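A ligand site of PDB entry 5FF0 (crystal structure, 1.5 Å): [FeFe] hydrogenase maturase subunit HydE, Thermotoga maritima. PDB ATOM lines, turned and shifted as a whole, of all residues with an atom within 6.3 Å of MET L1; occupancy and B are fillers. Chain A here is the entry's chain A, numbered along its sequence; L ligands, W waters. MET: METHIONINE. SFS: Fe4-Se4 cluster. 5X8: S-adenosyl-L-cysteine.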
ATOM      1  N   CYS A  73      20.625  14.973 -15.734  1.00  0.00           N
ATOM      2  CA  CYS A  73      20.452  14.241 -16.969  1.00  0.00           C
ATOM      3  C   CYS A  73      19.020  14.225 -17.455  1.00  0.00           C
ATOM      4  O   CYS A  73      18.115  14.059 -16.678  1.00  0.00           O
ATOM      5  CB  CYS A  73      20.931  12.767 -16.855  1.00  0.00           C
ATOM      6  SG  CYS A  73      21.189  11.993 -18.468  1.00  0.00           S
ATOM      7  N   CYS A  77      18.131   6.073 -18.603  1.00  0.00           N
ATOM      8  CA  CYS A  77      18.707   4.730 -18.732  1.00  0.00           C
ATOM      9  C   CYS A  77      18.411   3.909 -17.486  1.00  0.00           C
ATOM     10  O   CYS A  77      18.557   4.364 -16.370  1.00  0.00           O
ATOM     11  CB  CYS A  77      20.255   4.834 -18.983  1.00  0.00           C
ATOM     12  SG  CYS A  77      20.670   5.903 -20.368  1.00  0.00           S
ATOM     13  N   TYR A  79      19.705   1.477 -15.996  1.00  0.00           N
ATOM     14  CA  TYR A  79      20.815   1.024 -15.114  1.00  0.00           C
ATOM     15  C   TYR A  79      21.411   2.144 -14.268  1.00  0.00           C
ATOM     16  O   TYR A  79      22.086   1.915 -13.315  1.00  0.00           O
ATOM     17  CB  TYR A  79      21.917   0.362 -15.941  1.00  0.00           C
ATOM     18  CG  TYR A  79      22.294   1.094 -17.217  1.00  0.00           C
ATOM     19  CD1 TYR A  79      23.137   2.224 -17.177  1.00  0.00           C
ATOM     20  CD2 TYR A  79      21.816   0.687 -18.460  1.00  0.00           C
ATOM     21  CE1 TYR A  79      23.474   2.906 -18.342  1.00  0.00           C
ATOM     22  CE2 TYR A  79      22.143   1.393 -19.612  1.00  0.00           C
ATOM     23  CZ  TYR A  79      22.986   2.480 -19.545  1.00  0.00           C
ATOM     24  OH  TYR A  79      23.224   3.109 -20.676  1.00  0.00           O
ATOM     25  N   CYS A  80      21.236   3.396 -14.685  1.00  0.00           N
ATOM     26  CA  CYS A  80      22.007   4.502 -14.139  1.00  0.00           C
ATOM     27  C   CYS A  80      21.419   5.256 -12.961  1.00  0.00           C
ATOM     28  O   CYS A  80      20.313   5.655 -13.053  1.00  0.00           O
ATOM     29  CB  CYS A  80      22.209   5.478 -15.267  1.00  0.00           C
ATOM     30  SG  CYS A  80      23.337   6.858 -14.851  1.00  0.00           S
ATOM     31  N   LEU A  82      21.877   8.315 -12.183  1.00  0.00           N
ATOM     32  CA  LEU A  82      21.555   9.671 -12.552  1.00  0.00           C
ATOM     33  C   LEU A  82      20.308   9.808 -13.433  1.00  0.00           C
ATOM     34  O   LEU A  82      19.948  10.908 -13.792  1.00  0.00           O
ATOM     35  CB  LEU A  82      22.742  10.360 -13.257  1.00  0.00           C
ATOM     36  CG  LEU A  82      24.039  10.375 -12.515  1.00  0.00           C
ATOM     37  CD1 LEU A  82      25.046  11.254 -13.272  1.00  0.00           C
ATOM     38  CD2 LEU A  82      24.053  10.604 -11.093  1.00  0.00           C
ATOM     39  N   GLN A 117      33.069  15.053 -17.797  1.00  0.00           N
ATOM     40  CA  GLN A 117      31.959  14.120 -17.909  1.00  0.00           C
ATOM     41  C   GLN A 117      30.758  14.720 -17.201  1.00  0.00           C
ATOM     42  O   GLN A 117      30.886  15.386 -16.181  1.00  0.00           O
ATOM     43  CB  GLN A 117      32.275  12.769 -17.304  1.00  0.00           C
ATOM     44  CG  GLN A 117      31.236  11.709 -17.591  1.00  0.00           C
ATOM     45  CD  GLN A 117      31.546  10.320 -17.059  1.00  0.00           C
ATOM     46  OE1 GLN A 117      31.265  10.048 -15.930  1.00  0.00           O
ATOM     47  NE2 GLN A 117      32.082   9.504 -17.830  1.00  0.00           N
ATOM     48  N   SER A 118      29.584  14.422 -17.722  1.00  0.00           N
ATOM     49  CA  SER A 118      28.361  14.848 -17.074  1.00  0.00           C
ATOM     50  C   SER A 118      27.233  13.940 -17.491  1.00  0.00           C
ATOM     51  O   SER A 118      27.310  13.181 -18.453  1.00  0.00           O
ATOM     52  CB  SER A 118      28.028  16.315 -17.431  1.00  0.00           C
ATOM     53  OG  SER A 118      27.838  16.476 -18.818  1.00  0.00           O
ATOM     54  N   GLY A 119      26.107  14.091 -16.777  1.00  0.00           N
ATOM     55  CA  GLY A 119      24.813  13.693 -17.337  1.00  0.00           C
ATOM     56  C   GLY A 119      24.557  14.470 -18.612  1.00  0.00           C
ATOM     57  O   GLY A 119      25.243  15.474 -18.926  1.00  0.00           O
ATOM     58  N   GLU A 120      23.573  14.058 -19.392  1.00  0.00           N
ATOM     59  CA  GLU A 120      23.134  14.852 -20.526  1.00  0.00           C
ATOM     60  C   GLU A 120      22.374  16.066 -20.041  1.00  0.00           C
ATOM     61  O   GLU A 120      21.104  16.053 -19.976  1.00  0.00           O
ATOM     62  CB  GLU A 120      22.327  14.028 -21.515  1.00  0.00           C
ATOM     63  CG  GLU A 120      23.147  13.001 -22.263  1.00  0.00           C
ATOM     64  CD  GLU A 120      22.447  12.404 -23.460  1.00  0.00           C
ATOM     65  OE1 GLU A 120      21.351  12.878 -23.813  1.00  0.00           O
ATOM     66  OE2 GLU A 120      22.987  11.447 -24.059  1.00  0.00           O
ATOM     67  N   SER A 146      32.972  13.591 -22.337  1.00  0.00           N
ATOM     68  CA  SER A 146      32.090  12.398 -22.124  1.00  0.00           C
ATOM     69  C   SER A 146      30.726  12.971 -21.754  1.00  0.00           C
ATOM     70  O   SER A 146      30.403  12.941 -20.631  1.00  0.00           O
ATOM     71  CB  SER A 146      32.667  11.514 -21.055  1.00  0.00           C
ATOM     72  OG  SER A 146      31.963  10.288 -20.920  1.00  0.00           O
ATOM     73  N   LEU A 147      29.978  13.531 -22.704  1.00  0.00           N
ATOM     74  CA  LEU A 147      28.783  14.305 -22.453  1.00  0.00           C
ATOM     75  C   LEU A 147      27.518  13.623 -23.001  1.00  0.00           C
ATOM     76  O   LEU A 147      26.434  14.194 -22.859  1.00  0.00           O
ATOM     77  CB  LEU A 147      28.887  15.709 -23.005  1.00  0.00           C
ATOM     78  CG  LEU A 147      30.141  16.443 -22.670  1.00  0.00           C
ATOM     79  CD1 LEU A 147      30.195  17.843 -23.298  1.00  0.00           C
ATOM     80  CD2 LEU A 147      30.392  16.549 -21.186  1.00  0.00           C
ATOM     81  N   GLY A 148      27.648  12.450 -23.633  1.00  0.00           N
ATOM     82  CA  GLY A 148      26.463  11.783 -24.186  1.00  0.00           C
ATOM     83  C   GLY A 148      26.210  12.105 -25.645  1.00  0.00           C
ATOM     84  O   GLY A 148      27.106  12.494 -26.393  1.00  0.00           O
ATOM     85  N   GLU A 149      24.945  11.883 -26.000  1.00  0.00           N
ATOM     86  CA  GLU A 149      24.469  12.037 -27.401  1.00  0.00           C
ATOM     87  C   GLU A 149      23.918  13.438 -27.640  1.00  0.00           C
ATOM     88  O   GLU A 149      23.042  13.885 -26.974  1.00  0.00           O
ATOM     89  CB  GLU A 149      23.330  11.050 -27.616  1.00  0.00           C
ATOM     90  CG  GLU A 149      23.767   9.616 -27.459  1.00  0.00           C
ATOM     91  CD  GLU A 149      22.626   8.597 -27.455  1.00  0.00           C
ATOM     92  OE1 GLU A 149      21.625   8.794 -28.189  1.00  0.00           O
ATOM     93  OE2 GLU A 149      22.749   7.584 -26.752  1.00  0.00           O
ATOM     94  N   LEU A 167      34.520  10.197 -25.303  1.00  0.00           N
ATOM     95  CA  LEU A 167      34.112   8.887 -24.769  1.00  0.00           C
ATOM     96  C   LEU A 167      32.609   8.748 -24.889  1.00  0.00           C
ATOM     97  O   LEU A 167      31.836   9.516 -24.351  1.00  0.00           O
ATOM     98  CB  LEU A 167      34.492   8.725 -23.287  1.00  0.00           C
ATOM     99  CG  LEU A 167      35.933   9.103 -22.937  1.00  0.00           C
ATOM    100  CD1 LEU A 167      36.139   8.952 -21.426  1.00  0.00           C
ATOM    101  CD2 LEU A 167      36.889   8.284 -23.770  1.00  0.00           C
ATOM    102  N   LEU A 168      32.194   7.690 -25.587  1.00  0.00           N
ATOM    103  CA  LEU A 168      30.775   7.401 -25.715  1.00  0.00           C
ATOM    104  C   LEU A 168      30.625   5.876 -25.790  1.00  0.00           C
ATOM    105  O   LEU A 168      30.613   5.288 -26.857  1.00  0.00           O
ATOM    106  CB  LEU A 168      30.217   8.100 -26.952  1.00  0.00           C
ATOM    107  CG  LEU A 168      28.673   8.085 -27.069  1.00  0.00           C
ATOM    108  CD1 LEU A 168      28.068   9.032 -26.063  1.00  0.00           C
ATOM    109  CD2 LEU A 168      28.259   8.514 -28.501  1.00  0.00           C
ATOM    110  N   ARG A 169      30.516   5.249 -24.667  1.00  0.00           N
ATOM    111  CA  ARG A 169      30.444   3.810 -24.666  1.00  0.00           C
ATOM    112  C   ARG A 169      29.269   3.395 -25.476  1.00  0.00           C
ATOM    113  O   ARG A 169      28.223   3.997 -25.420  1.00  0.00           O
ATOM    114  CB  ARG A 169      30.279   3.326 -23.270  1.00  0.00           C
ATOM    115  CG  ARG A 169      31.578   3.338 -22.514  1.00  0.00           C
ATOM    116  CD  ARG A 169      31.347   2.655 -21.192  1.00  0.00           C
ATOM    117  NE  ARG A 169      32.451   2.827 -20.291  1.00  0.00           N
ATOM    118  CZ  ARG A 169      32.577   2.160 -19.166  1.00  0.00           C
ATOM    119  NH1 ARG A 169      31.647   1.314 -18.796  1.00  0.00           N
ATOM    120  NH2 ARG A 169      33.678   2.358 -18.440  1.00  0.00           N
ATOM    121  N   GLU A 171      27.688   0.669 -24.857  1.00  0.00           N
ATOM    122  CA  GLU A 171      26.887   0.100 -23.789  1.00  0.00           C
ATOM    123  C   GLU A 171      26.547  -1.394 -24.005  1.00  0.00           C
ATOM    124  O   GLU A 171      26.890  -2.224 -23.182  1.00  0.00           O
ATOM    125  CB  GLU A 171      25.626   0.917 -23.463  1.00  0.00           C
ATOM    126  CG  GLU A 171      25.871   2.397 -23.262  1.00  0.00           C
ATOM    127  CD  GLU A 171      26.818   2.762 -22.139  1.00  0.00           C
ATOM    128  OE1 GLU A 171      27.401   1.885 -21.499  1.00  0.00           O
ATOM    129  OE2 GLU A 171      26.947   4.006 -21.869  1.00  0.00           O
ATOM    130  N   ARG A 182      17.855   1.752 -22.629  1.00  0.00           N
ATOM    131  CA  ARG A 182      18.054   3.174 -22.896  1.00  0.00           C
ATOM    132  C   ARG A 182      16.857   3.630 -23.731  1.00  0.00           C
ATOM    133  O   ARG A 182      16.943   3.780 -24.903  1.00  0.00           O
ATOM    134  CB  ARG A 182      19.391   3.344 -23.632  1.00  0.00           C
ATOM    135  CG  ARG A 182      20.545   2.584 -22.942  1.00  0.00           C
ATOM    136  CD  ARG A 182      21.913   2.948 -23.499  1.00  0.00           C
ATOM    137  NE  ARG A 182      22.164   4.329 -23.191  1.00  0.00           N
ATOM    138  CZ  ARG A 182      22.281   5.274 -24.090  1.00  0.00           C
ATOM    139  NH1 ARG A 182      22.350   5.017 -25.367  1.00  0.00           N
ATOM    140  NH2 ARG A 182      22.350   6.524 -23.637  1.00  0.00           N
ATOM    141  N   ARG A 190      23.329   5.689 -31.173  1.00  0.00           N
ATOM    142  CA  ARG A 190      24.632   5.636 -30.491  1.00  0.00           C
ATOM    143  C   ARG A 190      25.761   5.444 -31.455  1.00  0.00           C
ATOM    144  O   ARG A 190      26.796   6.127 -31.421  1.00  0.00           O
ATOM    145  CB  ARG A 190      24.591   4.475 -29.467  1.00  0.00           C
ATOM    146  CG  ARG A 190      25.668   4.529 -28.370  1.00  0.00           C
ATOM    147  CD  ARG A 190      25.293   5.600 -27.362  1.00  0.00           C
ATOM    148  NE  ARG A 190      26.130   5.529 -26.151  1.00  0.00           N
ATOM    149  CZ  ARG A 190      26.038   6.403 -25.154  1.00  0.00           C
ATOM    150  NH1 ARG A 190      25.158   7.389 -25.189  1.00  0.00           N
ATOM    151  NH2 ARG A 190      26.882   6.312 -24.145  1.00  0.00           N
ATOM    152  N   TYR A 313      27.649  12.010  -7.546  1.00  0.00           N
ATOM    153  CA  TYR A 313      27.766  11.463  -8.865  1.00  0.00           C
ATOM    154  C   TYR A 313      28.053   9.986  -8.730  1.00  0.00           C
ATOM    155  O   TYR A 313      29.152   9.553  -8.776  1.00  0.00           O
ATOM    156  CB  TYR A 313      28.860  12.161  -9.673  1.00  0.00           C
ATOM    157  CG  TYR A 313      28.811  11.991 -11.166  1.00  0.00           C
ATOM    158  CD1 TYR A 313      28.267  12.965 -11.956  1.00  0.00           C
ATOM    159  CD2 TYR A 313      29.318  10.916 -11.766  1.00  0.00           C
ATOM    160  CE1 TYR A 313      28.248  12.867 -13.318  1.00  0.00           C
ATOM    161  CE2 TYR A 313      29.319  10.808 -13.119  1.00  0.00           C
ATOM    162  CZ  TYR A 313      28.763  11.799 -13.889  1.00  0.00           C
ATOM    163  OH  TYR A 313      28.776  11.692 -15.235  1.00  0.00           O
ATOM    164  N   LEU A 315      26.759   6.769 -10.444  1.00  0.00           N
ATOM    165  CA  LEU A 315      26.076   6.012 -11.474  1.00  0.00           C
ATOM    166  C   LEU A 315      25.710   4.646 -10.899  1.00  0.00           C
ATOM    167  O   LEU A 315      24.735   4.089 -11.246  1.00  0.00           O
ATOM    168  CB  LEU A 315      27.009   5.793 -12.664  1.00  0.00           C
ATOM    169  CG  LEU A 315      27.749   6.998 -13.186  1.00  0.00           C
ATOM    170  CD1 LEU A 315      28.637   6.631 -14.389  1.00  0.00           C
ATOM    171  CD2 LEU A 315      26.851   8.041 -13.534  1.00  0.00           C
HETATM  172  N   MET L   1      26.047  10.534 -19.967  1.00  0.00           N
HETATM  173  CA  MET L   1      27.254  10.183 -20.779  1.00  0.00           C
HETATM  174  C   MET L   1      26.918   8.890 -21.467  1.00  0.00           C
HETATM  175  O   MET L   1      27.649   8.520 -22.355  1.00  0.00           O
HETATM  176  CB  MET L   1      28.498  10.048 -19.861  1.00  0.00           C
HETATM  177  CG  MET L   1      28.608   8.691 -19.191  1.00  0.00           C
HETATM  178  SD  MET L   1      27.290   8.296 -17.989  1.00  0.00           S
HETATM  179  CE  MET L   1      27.778   9.563 -16.864  1.00  0.00           C
HETATM  180  OXT MET L   1      25.935   8.174 -21.055  1.00  0.00           O
HETATM  181 SE4  SFS L   2      20.849   8.246 -17.395  1.00  0.00          SE
HETATM  182 FE1  SFS L   2      23.184   7.952 -16.860  1.00  0.00          FE
HETATM  183 FE3  SFS L   2      22.100   7.434 -19.287  1.00  0.00          FE
HETATM  184 FE2  SFS L   2      22.150   9.986 -18.266  1.00  0.00          FE
HETATM  185 SE3  SFS L   2      24.161  10.023 -17.014  1.00  0.00          SE
HETATM  186 FE4  SFS L   2      24.787   8.836 -19.076  1.00  0.00          FE
HETATM  187 SE2  SFS L   2      24.173   6.474 -18.511  1.00  0.00          SE
HETATM  188 SE1  SFS L   2      22.726   9.325 -20.516  1.00  0.00          SE
HETATM  189  N1  5X8 L   3      27.008   0.113 -13.339  1.00  0.00           N
HETATM  190  C5  5X8 L   3      26.344   1.979 -14.474  1.00  0.00           C
HETATM  191  C8  5X8 L   3      26.423   3.599 -15.893  1.00  0.00           C
HETATM  192  C2  5X8 L   3      28.177   0.133 -13.989  1.00  0.00           C
HETATM  193  C6  5X8 L   3      26.079   1.048 -13.584  1.00  0.00           C
HETATM  194  N3  5X8 L   3      28.417   1.079 -14.865  1.00  0.00           N
HETATM  195  C4  5X8 L   3      27.525   1.972 -15.124  1.00  0.00           C
HETATM  196  O   5X8 L   3      33.082   4.663 -12.932  1.00  0.00           O
HETATM  197  C   5X8 L   3      33.572   4.108 -13.930  1.00  0.00           C
HETATM  198  OXT 5X8 L   3      33.822   2.965 -14.058  1.00  0.00           O
HETATM  199  CA  5X8 L   3      33.583   4.973 -15.171  1.00  0.00           C
HETATM  200  N   5X8 L   3      34.675   4.474 -16.018  1.00  0.00           N
HETATM  201  CB  5X8 L   3      32.205   5.010 -15.812  1.00  0.00           C
HETATM  202  SG  5X8 L   3      32.214   6.023 -17.391  1.00  0.00           S
HETATM  203  C5' 5X8 L   3      30.349   6.027 -17.920  1.00  0.00           C
HETATM  204  C4' 5X8 L   3      29.787   4.690 -18.126  1.00  0.00           C
HETATM  205  O4' 5X8 L   3      29.413   4.205 -16.853  1.00  0.00           O
HETATM  206  C3' 5X8 L   3      28.473   4.690 -18.870  1.00  0.00           C
HETATM  207  O3' 5X8 L   3      28.763   4.807 -20.269  1.00  0.00           O
HETATM  208  C2' 5X8 L   3      28.033   3.267 -18.453  1.00  0.00           C
HETATM  209  O2' 5X8 L   3      28.664   2.216 -19.244  1.00  0.00           O
HETATM  210  C1' 5X8 L   3      28.614   3.109 -17.007  1.00  0.00           C
HETATM  211  N9  5X8 L   3      27.590   2.921 -16.017  1.00  0.00           N
HETATM  212  N7  5X8 L   3      25.683   3.027 -14.949  1.00  0.00           N
HETATM  213  N6  5X8 L   3      24.977   1.008 -12.887  1.00  0.00           N
HETATM  214  O   HOH W   1      24.329   9.281 -23.323  1.00  0.00           O
HETATM  215  O   HOH W   2      24.673   5.440 -21.509  1.00  0.00           O
HETATM  216  O   HOH W   3      29.591  10.336 -23.192  1.00  0.00           O
HETATM  217  O   HOH W   4      29.802   6.578 -22.045  1.00  0.00           O
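The guanidinium group (NH2) of Arg 190 is in salt-bridge range of an oxygen (O) of MET L1, at 2.9 Å. The backbone carbonyl oxygen (O) of Ser 118 lies close to a nitrogen (N) of MET L1. An iron atom (FE1) of SFS L2 is bound by the side-chain sulfur (SG) of Cys 80, 2.3 Å away. The side-chain sulfur of Cys 73 binds an iron atom (FE2) of SFS L2. FE3 of SFS L2 is bound by SG of Cys 77. The side-chain amide nitrogen (NE2) of Gln 117 lies close to a sulfur (SG) of 5X8 L3 (3.5 Å). The backbone carbonyl oxygen (O) of Leu 315 is in hydrogen-bond range of a nitrogen (N6) of 5X8 L3, at 3.5 Å. OE2 of Glu 171 lies within hydrogen-bond range of O3' of 5X8 L3. An oxygen (O2') of 5X8 L3 sits at hydrogen-bond distance from the guanidinium group of Arg 169, 3.1 Å away. N6 of 5X8 L3 sits at hydrogen-bond distance from O of Tyr 79 (3.1 Å).
An iron atom (FE4) of SFS L2 is bound by a nitrogen (N) of MET L1, 2.3 Å away.
OH of Tyr 313 sits at hydrogen-bond distance from OE1 of Gln 117. The side-chain carboxylate (OE2) of Glu 171 is in salt-bridge range of the guanidinium group (NH2) of Arg 190. The backbone carbonyl oxygen of Arg 169 lies within hydrogen-bond range of the guanidinium group of Arg 190. The guanidinium group of Arg 190 is in salt-bridge range of the side-chain carboxylate of Glu 149 (2.9 Å). The backbone NH (N) of Ser 118 sits at hydrogen-bond distance from the backbone carbonyl oxygen (O) of Ser 146 (3.4 Å). The side-chain hydroxyl (OG) of Ser 146 lies within hydrogen-bond range of the side-chain amide nitrogen (NE2) of Gln 117 (3.2 Å).
Gln 117 touches MET L1. O of Ser 146 touches CB of MET L1, at 3.5 Å. Gly 148 touches MET L1. Leu 168 touches MET L1 (CD1 to O, 3.8 Å). Tyr 313 touches MET L1. CD2 of Leu 315 touches CE of MET L1 (3.8 Å). Along chain A the residues within 4 Å of MET L1 span positions 117 to 315.
Water W3 lies within hydrogen-bond range of O of Leu 167 (2.7 Å), O of MET L1 (2.8 Å), N of Gly 148 (2.9 Å), N of Leu 147 (3.3 Å) and OG of Ser 146 (3.3 Å). Water W4 lies within hydrogen-bond range of O3' of 5X8 L3 (2.7 Å), O of MET L1 (2.9 Å) and N of Arg 169 (3.0 Å). Water W1 lies within hydrogen-bond range of the side-chain carboxylate of Glu 120 (2.7 Å), the guanidinium group of Arg 190 (2.8 Å) and the guanidinium group of Arg 182 (3.4 Å). Water W2 lies within hydrogen-bond range of the side-chain carboxylate of Glu 171 (2.7 Å), the side-chain hydroxyl of Tyr 79 (2.9 Å) and the guanidinium group of Arg 182 (3.2 Å).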
